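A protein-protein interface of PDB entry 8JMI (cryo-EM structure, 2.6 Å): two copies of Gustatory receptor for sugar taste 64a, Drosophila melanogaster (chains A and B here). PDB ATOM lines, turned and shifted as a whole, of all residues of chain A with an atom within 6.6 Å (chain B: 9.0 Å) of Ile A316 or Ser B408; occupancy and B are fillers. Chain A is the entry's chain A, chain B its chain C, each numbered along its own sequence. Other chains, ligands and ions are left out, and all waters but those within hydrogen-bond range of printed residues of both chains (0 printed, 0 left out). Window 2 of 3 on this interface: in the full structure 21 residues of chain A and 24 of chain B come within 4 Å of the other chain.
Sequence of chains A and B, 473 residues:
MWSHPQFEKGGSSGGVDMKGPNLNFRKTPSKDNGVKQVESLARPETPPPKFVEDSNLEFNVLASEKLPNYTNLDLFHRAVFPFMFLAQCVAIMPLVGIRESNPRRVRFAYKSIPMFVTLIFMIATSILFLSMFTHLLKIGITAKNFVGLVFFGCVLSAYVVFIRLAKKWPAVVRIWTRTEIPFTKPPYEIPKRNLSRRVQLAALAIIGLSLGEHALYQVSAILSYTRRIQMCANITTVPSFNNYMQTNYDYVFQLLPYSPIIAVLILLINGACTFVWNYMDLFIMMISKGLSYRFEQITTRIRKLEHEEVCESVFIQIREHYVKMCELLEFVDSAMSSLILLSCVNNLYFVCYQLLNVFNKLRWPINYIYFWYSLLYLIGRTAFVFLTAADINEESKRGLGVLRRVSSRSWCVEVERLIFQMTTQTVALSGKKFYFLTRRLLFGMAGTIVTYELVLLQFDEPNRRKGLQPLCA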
ATOM      1  N   CYS A 311      41.322  12.022  -5.222  1.00  0.00           N
ATOM      2  CA  CYS A 311      41.112  11.513  -6.566  1.00  0.00           C
ATOM      3  C   CYS A 311      39.662  11.719  -6.994  1.00  0.00           C
ATOM      4  O   CYS A 311      38.765  11.928  -6.174  1.00  0.00           O
ATOM      5  CB  CYS A 311      41.475  10.030  -6.643  1.00  0.00           C
ATOM      6  SG  CYS A 311      41.115   9.100  -5.136  1.00  0.00           S
ATOM      7  N   GLU A 312      39.441  11.658  -8.308  1.00  0.00           N
ATOM      8  CA  GLU A 312      38.101  11.880  -8.839  1.00  0.00           C
ATOM      9  C   GLU A 312      37.121  10.820  -8.355  1.00  0.00           C
ATOM     10  O   GLU A 312      35.930  11.105  -8.204  1.00  0.00           O
ATOM     11  CB  GLU A 312      38.139  11.905 -10.367  1.00  0.00           C
ATOM     12  CG  GLU A 312      36.839  12.376 -11.012  1.00  0.00           C
ATOM     13  CD  GLU A 312      37.026  13.551 -11.958  1.00  0.00           C
ATOM     14  OE1 GLU A 312      38.174  13.819 -12.375  1.00  0.00           O
ATOM     15  OE2 GLU A 312      36.019  14.212 -12.289  1.00  0.00           O
ATOM     16  N   SER A 313      37.596   9.596  -8.111  1.00  0.00           N
ATOM     17  CA  SER A 313      36.698   8.524  -7.693  1.00  0.00           C
ATOM     18  C   SER A 313      36.075   8.815  -6.333  1.00  0.00           C
ATOM     19  O   SER A 313      34.899   8.508  -6.098  1.00  0.00           O
ATOM     20  CB  SER A 313      37.452   7.195  -7.662  1.00  0.00           C
ATOM     21  OG  SER A 313      38.454   7.204  -6.661  1.00  0.00           O
ATOM     22  N   VAL A 314      36.853   9.390  -5.415  1.00  0.00           N
ATOM     23  CA  VAL A 314      36.322   9.724  -4.096  1.00  0.00           C
ATOM     24  C   VAL A 314      35.183  10.726  -4.227  1.00  0.00           C
ATOM     25  O   VAL A 314      34.126  10.580  -3.602  1.00  0.00           O
ATOM     26  CB  VAL A 314      37.444  10.260  -3.188  1.00  0.00           C
ATOM     27  CG1 VAL A 314      36.861  10.931  -1.952  1.00  0.00           C
ATOM     28  CG2 VAL A 314      38.390   9.138  -2.797  1.00  0.00           C
ATOM     29  N   PHE A 315      35.381  11.759  -5.047  1.00  0.00           N
ATOM     30  CA  PHE A 315      34.323  12.740  -5.262  1.00  0.00           C
ATOM     31  C   PHE A 315      33.130  12.116  -5.970  1.00  0.00           C
ATOM     32  O   PHE A 315      31.984  12.483  -5.697  1.00  0.00           O
ATOM     33  CB  PHE A 315      34.860  13.925  -6.063  1.00  0.00           C
ATOM     34  CG  PHE A 315      35.791  14.807  -5.288  1.00  0.00           C
ATOM     35  CD1 PHE A 315      35.415  15.328  -4.061  1.00  0.00           C
ATOM     36  CD2 PHE A 315      37.041  15.122  -5.789  1.00  0.00           C
ATOM     37  CE1 PHE A 315      36.269  16.141  -3.349  1.00  0.00           C
ATOM     38  CE2 PHE A 315      37.897  15.938  -5.081  1.00  0.00           C
ATOM     39  CZ  PHE A 315      37.511  16.447  -3.859  1.00  0.00           C
ATOM     40  N   ILE A 316      33.375  11.178  -6.886  1.00  0.00           N
ATOM     41  CA  ILE A 316      32.273  10.486  -7.547  1.00  0.00           C
ATOM     42  C   ILE A 316      31.414   9.771  -6.515  1.00  0.00           C
ATOM     43  O   ILE A 316      30.183   9.886  -6.514  1.00  0.00           O
ATOM     44  CB  ILE A 316      32.808   9.502  -8.603  1.00  0.00           C
ATOM     45  CG1 ILE A 316      33.375  10.261  -9.804  1.00  0.00           C
ATOM     46  CG2 ILE A 316      31.704   8.546  -9.042  1.00  0.00           C
ATOM     47  CD1 ILE A 316      34.156   9.397 -10.770  1.00  0.00           C
ATOM     48  N   GLN A 317      32.056   9.018  -5.620  1.00  0.00           N
ATOM     49  CA  GLN A 317      31.306   8.283  -4.606  1.00  0.00           C
ATOM     50  C   GLN A 317      30.582   9.233  -3.661  1.00  0.00           C
ATOM     51  O   GLN A 317      29.431   8.986  -3.284  1.00  0.00           O
ATOM     52  CB  GLN A 317      32.236   7.358  -3.823  1.00  0.00           C
ATOM     53  CG  GLN A 317      31.502   6.484  -2.818  1.00  0.00           C
ATOM     54  CD  GLN A 317      32.373   5.389  -2.242  1.00  0.00           C
ATOM     55  OE1 GLN A 317      33.069   5.590  -1.246  1.00  0.00           O
ATOM     56  NE2 GLN A 317      32.335   4.216  -2.862  1.00  0.00           N
ATOM     57  N   ILE A 318      31.237  10.324  -3.263  1.00  0.00           N
ATOM     58  CA  ILE A 318      30.605  11.275  -2.352  1.00  0.00           C
ATOM     59  C   ILE A 318      29.377  11.896  -3.005  1.00  0.00           C
ATOM     60  O   ILE A 318      28.315  12.013  -2.383  1.00  0.00           O
ATOM     61  CB  ILE A 318      31.615  12.350  -1.910  1.00  0.00           C
ATOM     62  CG1 ILE A 318      32.713  11.719  -1.055  1.00  0.00           C
ATOM     63  CG2 ILE A 318      30.908  13.457  -1.136  1.00  0.00           C
ATOM     64  CD1 ILE A 318      33.876  12.638  -0.767  1.00  0.00           C
ATOM     65  N   ARG A 319      29.505  12.306  -4.268  1.00  0.00           N
ATOM     66  CA  ARG A 319      28.377  12.913  -4.965  1.00  0.00           C
ATOM     67  C   ARG A 319      27.249  11.909  -5.156  1.00  0.00           C
ATOM     68  O   ARG A 319      26.072  12.259  -5.026  1.00  0.00           O
ATOM     69  CB  ARG A 319      28.831  13.471  -6.314  1.00  0.00           C
ATOM     70  CG  ARG A 319      27.834  14.430  -6.950  1.00  0.00           C
ATOM     71  CD  ARG A 319      28.207  14.788  -8.379  1.00  0.00           C
ATOM     72  NE  ARG A 319      28.350  13.608  -9.224  1.00  0.00           N
ATOM     73  CZ  ARG A 319      27.336  12.882  -9.673  1.00  0.00           C
ATOM     74  NH1 ARG A 319      26.082  13.186  -9.379  1.00  0.00           N
ATOM     75  NH2 ARG A 319      27.586  11.821 -10.436  1.00  0.00           N
ATOM     76  N   GLU A 320      27.584  10.656  -5.472  1.00  0.00           N
ATOM     77  CA  GLU A 320      26.550   9.644  -5.645  1.00  0.00           C
ATOM     78  C   GLU A 320      25.811   9.382  -4.340  1.00  0.00           C
ATOM     79  O   GLU A 320      24.581   9.263  -4.327  1.00  0.00           O
ATOM     80  CB  GLU A 320      27.167   8.353  -6.182  1.00  0.00           C
ATOM     81  CG  GLU A 320      27.518   8.416  -7.660  1.00  0.00           C
ATOM     82  CD  GLU A 320      28.269   7.189  -8.139  1.00  0.00           C
ATOM     83  OE1 GLU A 320      28.848   6.474  -7.295  1.00  0.00           O
ATOM     84  OE2 GLU A 320      28.278   6.940  -9.364  1.00  0.00           O
ATOM     85  N   HIS A 321      26.543   9.294  -3.227  1.00  0.00           N
ATOM     86  CA  HIS A 321      25.898   9.097  -1.934  1.00  0.00           C
ATOM     87  C   HIS A 321      25.036  10.295  -1.557  1.00  0.00           C
ATOM     88  O   HIS A 321      23.937  10.131  -1.020  1.00  0.00           O
ATOM     89  CB  HIS A 321      26.951   8.830  -0.861  1.00  0.00           C
ATOM     90  CG  HIS A 321      27.588   7.480  -0.968  1.00  0.00           C
ATOM     91  ND1 HIS A 321      28.756   7.155  -0.314  1.00  0.00           N
ATOM     92  CD2 HIS A 321      27.218   6.371  -1.649  1.00  0.00           C
ATOM     93  CE1 HIS A 321      29.080   5.904  -0.590  1.00  0.00           C
ATOM     94  NE2 HIS A 321      28.162   5.406  -1.399  1.00  0.00           N
ATOM     95  N   CYS A 412      37.752  19.076  -9.897  1.00  0.00           N
ATOM     96  CA  CYS A 412      37.335  18.382 -11.104  1.00  0.00           C
ATOM     97  C   CYS A 412      35.856  18.666 -11.339  1.00  0.00           C
ATOM     98  O   CYS A 412      35.213  19.393 -10.579  1.00  0.00           O
ATOM     99  CB  CYS A 412      37.606  16.877 -11.002  1.00  0.00           C
ATOM    100  SG  CYS A 412      36.838  16.067  -9.583  1.00  0.00           S
ATOM    101  N   VAL A 413      35.319  18.075 -12.407  1.00  0.00           N
ATOM    102  CA  VAL A 413      33.917  18.291 -12.746  1.00  0.00           C
ATOM    103  C   VAL A 413      33.008  17.735 -11.660  1.00  0.00           C
ATOM    104  O   VAL A 413      31.918  18.267 -11.423  1.00  0.00           O
ATOM    105  CB  VAL A 413      33.606  17.667 -14.121  1.00  0.00           C
ATOM    106  CG1 VAL A 413      32.141  17.259 -14.220  1.00  0.00           C
ATOM    107  CG2 VAL A 413      33.965  18.638 -15.233  1.00  0.00           C
ATOM    108  N   GLU A 414      33.423  16.658 -10.992  1.00  0.00           N
ATOM    109  CA  GLU A 414      32.583  16.063  -9.957  1.00  0.00           C
ATOM    110  C   GLU A 414      32.413  17.004  -8.770  1.00  0.00           C
ATOM    111  O   GLU A 414      31.308  17.146  -8.234  1.00  0.00           O
ATOM    112  CB  GLU A 414      33.180  14.732  -9.509  1.00  0.00           C
ATOM    113  CG  GLU A 414      33.168  13.673 -10.590  1.00  0.00           C
ATOM    114  CD  GLU A 414      31.765  13.267 -10.996  1.00  0.00           C
ATOM    115  OE1 GLU A 414      30.999  12.810 -10.122  1.00  0.00           O
ATOM    116  OE2 GLU A 414      31.425  13.410 -12.190  1.00  0.00           O
ATOM    117  N   ARG A 417      30.031  19.740  -9.821  1.00  0.00           N
ATOM    118  CA  ARG A 417      28.654  19.257  -9.803  1.00  0.00           C
ATOM    119  C   ARG A 417      28.114  19.204  -8.381  1.00  0.00           C
ATOM    120  O   ARG A 417      27.007  19.683  -8.100  1.00  0.00           O
ATOM    121  CB  ARG A 417      28.579  17.869 -10.438  1.00  0.00           C
ATOM    122  CG  ARG A 417      28.559  17.841 -11.948  1.00  0.00           C
ATOM    123  CD  ARG A 417      28.429  16.410 -12.437  1.00  0.00           C
ATOM    124  NE  ARG A 417      27.094  15.872 -12.198  1.00  0.00           N
ATOM    125  CZ  ARG A 417      26.655  14.712 -12.665  1.00  0.00           C
ATOM    126  NH1 ARG A 417      27.424  13.924 -13.398  1.00  0.00           N
ATOM    127  NH2 ARG A 417      25.410  14.332 -12.390  1.00  0.00           N
ATOM    128  N   GLU B 308      20.880   4.754 -17.807  1.00  0.00           N
ATOM    129  CA  GLU B 308      21.467   4.512 -19.114  1.00  0.00           C
ATOM    130  C   GLU B 308      22.549   5.544 -19.391  1.00  0.00           C
ATOM    131  O   GLU B 308      22.466   6.690 -18.942  1.00  0.00           O
ATOM    132  CB  GLU B 308      20.408   4.571 -20.224  1.00  0.00           C
ATOM    133  CG  GLU B 308      19.158   3.759 -19.936  1.00  0.00           C
ATOM    134  CD  GLU B 308      18.178   3.773 -21.094  1.00  0.00           C
ATOM    135  OE1 GLU B 308      18.446   4.476 -22.091  1.00  0.00           O
ATOM    136  OE2 GLU B 308      17.142   3.082 -21.007  1.00  0.00           O
ATOM    137  N   GLU B 309      23.569   5.124 -20.135  1.00  0.00           N
ATOM    138  CA  GLU B 309      24.565   6.052 -20.659  1.00  0.00           C
ATOM    139  C   GLU B 309      23.934   6.799 -21.826  1.00  0.00           C
ATOM    140  O   GLU B 309      23.458   6.180 -22.784  1.00  0.00           O
ATOM    141  CB  GLU B 309      25.826   5.307 -21.090  1.00  0.00           C
ATOM    142  CG  GLU B 309      26.532   4.568 -19.963  1.00  0.00           C
ATOM    143  CD  GLU B 309      26.860   5.470 -18.788  1.00  0.00           C
ATOM    144  OE1 GLU B 309      27.357   6.591 -19.018  1.00  0.00           O
ATOM    145  OE2 GLU B 309      26.623   5.055 -17.633  1.00  0.00           O
ATOM    146  N   VAL B 310      23.927   8.125 -21.749  1.00  0.00           N
ATOM    147  CA  VAL B 310      23.180   8.965 -22.676  1.00  0.00           C
ATOM    148  C   VAL B 310      24.161   9.734 -23.548  1.00  0.00           C
ATOM    149  O   VAL B 310      25.078  10.390 -23.038  1.00  0.00           O
ATOM    150  CB  VAL B 310      22.249   9.926 -21.919  1.00  0.00           C
ATOM    151  CG1 VAL B 310      21.373  10.698 -22.888  1.00  0.00           C
ATOM    152  CG2 VAL B 310      21.398   9.162 -20.915  1.00  0.00           C
ATOM    153  N   PHE B 315      20.742  14.651 -24.954  1.00  0.00           N
ATOM    154  CA  PHE B 315      20.674  15.819 -24.086  1.00  0.00           C
ATOM    155  C   PHE B 315      20.456  17.092 -24.891  1.00  0.00           C
ATOM    156  O   PHE B 315      19.764  18.006 -24.435  1.00  0.00           O
ATOM    157  CB  PHE B 315      21.948  15.929 -23.250  1.00  0.00           C
ATOM    158  CG  PHE B 315      22.057  14.892 -22.173  1.00  0.00           C
ATOM    159  CD1 PHE B 315      21.030  14.708 -21.263  1.00  0.00           C
ATOM    160  CD2 PHE B 315      23.188  14.105 -22.067  1.00  0.00           C
ATOM    161  CE1 PHE B 315      21.129  13.757 -20.271  1.00  0.00           C
ATOM    162  CE2 PHE B 315      23.294  13.154 -21.076  1.00  0.00           C
ATOM    163  CZ  PHE B 315      22.261  12.979 -20.176  1.00  0.00           C
ATOM    164  N   LEU B 403      18.276  14.569 -13.582  1.00  0.00           N
ATOM    165  CA  LEU B 403      19.475  15.060 -14.252  1.00  0.00           C
ATOM    166  C   LEU B 403      20.682  15.032 -13.325  1.00  0.00           C
ATOM    167  O   LEU B 403      21.817  14.875 -13.790  1.00  0.00           O
ATOM    168  CB  LEU B 403      19.243  16.478 -14.776  1.00  0.00           C
ATOM    169  CG  LEU B 403      18.387  16.618 -16.037  1.00  0.00           C
ATOM    170  CD1 LEU B 403      18.266  18.080 -16.426  1.00  0.00           C
ATOM    171  CD2 LEU B 403      18.963  15.806 -17.187  1.00  0.00           C
ATOM    172  N   ARG B 404      20.462  15.184 -12.018  1.00  0.00           N
ATOM    173  CA  ARG B 404      21.561  15.110 -11.064  1.00  0.00           C
ATOM    174  C   ARG B 404      22.127  13.703 -10.943  1.00  0.00           C
ATOM    175  O   ARG B 404      23.224  13.534 -10.403  1.00  0.00           O
ATOM    176  CB  ARG B 404      21.097  15.600  -9.692  1.00  0.00           C
ATOM    177  CG  ARG B 404      20.882  17.100  -9.611  1.00  0.00           C
ATOM    178  CD  ARG B 404      19.830  17.452  -8.577  1.00  0.00           C
ATOM    179  NE  ARG B 404      19.758  18.889  -8.344  1.00  0.00           N
ATOM    180  CZ  ARG B 404      18.688  19.527  -7.888  1.00  0.00           C
ATOM    181  NH1 ARG B 404      17.570  18.883  -7.593  1.00  0.00           N
ATOM    182  NH2 ARG B 404      18.741  20.845  -7.723  1.00  0.00           N
ATOM    183  N   ARG B 405      21.407  12.695 -11.429  1.00  0.00           N
ATOM    184  CA  ARG B 405      21.863  11.313 -11.392  1.00  0.00           C
ATOM    185  C   ARG B 405      22.655  10.920 -12.631  1.00  0.00           C
ATOM    186  O   ARG B 405      23.094   9.769 -12.727  1.00  0.00           O
ATOM    187  CB  ARG B 405      20.668  10.370 -11.232  1.00  0.00           C
ATOM    188  CG  ARG B 405      20.071  10.357  -9.834  1.00  0.00           C
ATOM    189  CD  ARG B 405      18.658   9.788  -9.826  1.00  0.00           C
ATOM    190  NE  ARG B 405      17.737  10.624  -9.066  1.00  0.00           N
ATOM    191  CZ  ARG B 405      16.421  10.637  -9.230  1.00  0.00           C
ATOM    192  NH1 ARG B 405      15.826   9.863 -10.123  1.00  0.00           N
ATOM    193  NH2 ARG B 405      15.681  11.447  -8.477  1.00  0.00           N
ATOM    194  N   VAL B 406      22.844  11.840 -13.579  1.00  0.00           N
ATOM    195  CA  VAL B 406      23.596  11.520 -14.784  1.00  0.00           C
ATOM    196  C   VAL B 406      25.002  11.082 -14.403  1.00  0.00           C
ATOM    197  O   VAL B 406      25.644  11.670 -13.523  1.00  0.00           O
ATOM    198  CB  VAL B 406      23.618  12.731 -15.733  1.00  0.00           C
ATOM    199  CG1 VAL B 406      24.720  12.581 -16.772  1.00  0.00           C
ATOM    200  CG2 VAL B 406      22.266  12.899 -16.404  1.00  0.00           C
ATOM    201  N   SER B 407      25.486  10.040 -15.069  1.00  0.00           N
ATOM    202  CA  SER B 407      26.783   9.476 -14.737  1.00  0.00           C
ATOM    203  C   SER B 407      27.907  10.427 -15.137  1.00  0.00           C
ATOM    204  O   SER B 407      27.732  11.340 -15.949  1.00  0.00           O
ATOM    205  CB  SER B 407      26.975   8.128 -15.431  1.00  0.00           C
ATOM    206  OG  SER B 407      26.878   8.261 -16.837  1.00  0.00           O
ATOM    207  N   SER B 408      29.082  10.198 -14.548  1.00  0.00           N
ATOM    208  CA  SER B 408      30.246  11.005 -14.892  1.00  0.00           C
ATOM    209  C   SER B 408      30.631  10.830 -16.353  1.00  0.00           C
ATOM    210  O   SER B 408      31.132  11.770 -16.979  1.00  0.00           O
ATOM    211  CB  SER B 408      31.422  10.635 -13.987  1.00  0.00           C
ATOM    212  OG  SER B 408      30.975  10.310 -12.683  1.00  0.00           O
ATOM    213  N   ARG B 409      30.410   9.640 -16.912  1.00  0.00           N
ATOM    214  CA  ARG B 409      30.728   9.402 -18.315  1.00  0.00           C
ATOM    215  C   ARG B 409      29.757  10.127 -19.238  1.00  0.00           C
ATOM    216  O   ARG B 409      30.168  10.675 -20.266  1.00  0.00           O
ATOM    217  CB  ARG B 409      30.719   7.899 -18.601  1.00  0.00           C
ATOM    218  CG  ARG B 409      30.850   7.540 -20.078  1.00  0.00           C
ATOM    219  CD  ARG B 409      30.909   6.032 -20.310  1.00  0.00           C
ATOM    220  NE  ARG B 409      31.210   5.278 -19.098  1.00  0.00           N
ATOM    221  CZ  ARG B 409      32.432   4.973 -18.682  1.00  0.00           C
ATOM    222  NH1 ARG B 409      33.508   5.348 -19.356  1.00  0.00           N
ATOM    223  NH2 ARG B 409      32.580   4.275 -17.561  1.00  0.00           N
ATOM    224  N   SER B 410      28.470  10.139 -18.890  1.00  0.00           N
ATOM    225  CA  SER B 410      27.461  10.789 -19.715  1.00  0.00           C
ATOM    226  C   SER B 410      27.402  12.296 -19.507  1.00  0.00           C
ATOM    227  O   SER B 410      26.789  12.992 -20.322  1.00  0.00           O
ATOM    228  CB  SER B 410      26.084  10.185 -19.427  1.00  0.00           C
ATOM    229  OG  SER B 410      25.932   8.932 -20.070  1.00  0.00           O
ATOM    230  N   TRP B 411      28.016  12.811 -18.447  1.00  0.00           N
ATOM    231  CA  TRP B 411      27.972  14.241 -18.181  1.00  0.00           C
ATOM    232  C   TRP B 411      28.684  15.011 -19.285  1.00  0.00           C
ATOM    233  O   TRP B 411      29.782  14.645 -19.714  1.00  0.00           O
ATOM    234  CB  TRP B 411      28.616  14.544 -16.831  1.00  0.00           C
ATOM    235  CG  TRP B 411      28.569  15.987 -16.447  1.00  0.00           C
ATOM    236  CD1 TRP B 411      29.567  16.905 -16.587  1.00  0.00           C
ATOM    237  CD2 TRP B 411      27.468  16.681 -15.847  1.00  0.00           C
ATOM    238  NE1 TRP B 411      29.158  18.127 -16.116  1.00  0.00           N
ATOM    239  CE2 TRP B 411      27.873  18.016 -15.654  1.00  0.00           C
ATOM    240  CE3 TRP B 411      26.182  16.302 -15.454  1.00  0.00           C
ATOM    241  CZ2 TRP B 411      27.037  18.974 -15.089  1.00  0.00           C
ATOM    242  CZ3 TRP B 411      25.353  17.255 -14.892  1.00  0.00           C
ATOM    243  CH2 TRP B 411      25.785  18.575 -14.715  1.00  0.00           C
ATOM    244  N   CYS B 412      28.052  16.088 -19.744  1.00  0.00           N
ATOM    245  CA  CYS B 412      28.611  16.922 -20.797  1.00  0.00           C
ATOM    246  C   CYS B 412      28.139  18.353 -20.583  1.00  0.00           C
ATOM    247  O   CYS B 412      27.415  18.657 -19.631  1.00  0.00           O
ATOM    248  CB  CYS B 412      28.217  16.403 -22.184  1.00  0.00           C
ATOM    249  SG  CYS B 412      26.438  16.252 -22.454  1.00  0.00           S
ATOM    250  N   VAL B 415      24.218  18.787 -20.486  1.00  0.00           N
ATOM    251  CA  VAL B 415      23.551  18.492 -19.220  1.00  0.00           C
ATOM    252  C   VAL B 415      23.782  19.624 -18.233  1.00  0.00           C
ATOM    253  O   VAL B 415      22.880  19.999 -17.476  1.00  0.00           O
ATOM    254  CB  VAL B 415      24.025  17.143 -18.643  1.00  0.00           C
ATOM    255  CG1 VAL B 415      22.983  16.591 -17.685  1.00  0.00           C
ATOM    256  CG2 VAL B 415      24.295  16.142 -19.746  1.00  0.00           C
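The guanidinium group (NH1) of Arg A417 sits at hydrogen-bond distance from the backbone carbonyl oxygen (O) of Val B406 (2.9 Å). O of Arg B404 sits at hydrogen-bond distance from NH1 of Arg A319 (3.1 Å). The side-chain hydroxyl of Ser B408 is in hydrogen-bond range of the side-chain carboxylate of Glu A414 (3.2 Å). The guanidinium group of Arg A417 sits at hydrogen-bond distance from the backbone carbonyl oxygen of Arg B404 (3.1 Å).
The guanidinium group of Arg A319 is in salt-bridge range of the side-chain carboxylate of Glu A414 (2.9 Å). The side-chain hydroxyl (OG) of Ser B407 is in hydrogen-bond range of the side-chain carboxylate (OE1) of Glu B309. The side-chain sulfur (SG) of Cys A412 lies close to the backbone NH (N) of Glu A414, 3.7 Å away. N of Ser B410 sits at hydrogen-bond distance from OG of Ser B407 (3.2 Å).
Of the 15 printed residues of chain B, 6 touch a printed residue of chain A. Printed residues of chain B that touch a printed residue of chain A: Leu B403, Arg B404, Val B406, Ser B407, Ser B408 and Trp B411. Hydrophobic or aromatic side chains of chain B within 4 Å of the printed part of chain A: Trp B411. Hydrophobic or aromatic side chains of chain A within 4 Å of the printed part of chain B: Ile A316 and Val A413. Among the printed residues, 10 pairs touch across the chains. Among the printed residues, no Asp or Glu carboxylate lies within 4 Å of a Lys or Arg side-chain nitrogen of the other chain.
Among the printed residues, pairs that only touch across the chains: Arg A417 with Trp B411 (3.2 Å), Val A413 with Trp B411 (3.5 Å), Arg A417 with Ser B407 (3.6 Å), Arg A319 with Val B406 (3.7 Å), Ile A316 with Ser B408 (3.7 Å) and Arg A417 with Leu B403 (3.9 Å).
Of the printed residues of chain B, Ile A316 touches Ser B408. Printed residues of chain A within 4 Å of Leu B403: Arg A417. Printed residues of chain A within 4 Å of Val B406: Arg A319 (3.7 Å) and Arg A417 (2.9 Å). Of the printed residues of chain A, Trp B411 touches Val A413 (3.5 Å) and Arg A417 (3.2 Å). The nearest residue of chain A that does not touch Ser B408 is Arg A417 (4.2 Å).
2 positions are printed for both chains. Of the 10 pairs that touch across the chains among the printed residues, none has its exchanged pair printed and touching as well.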
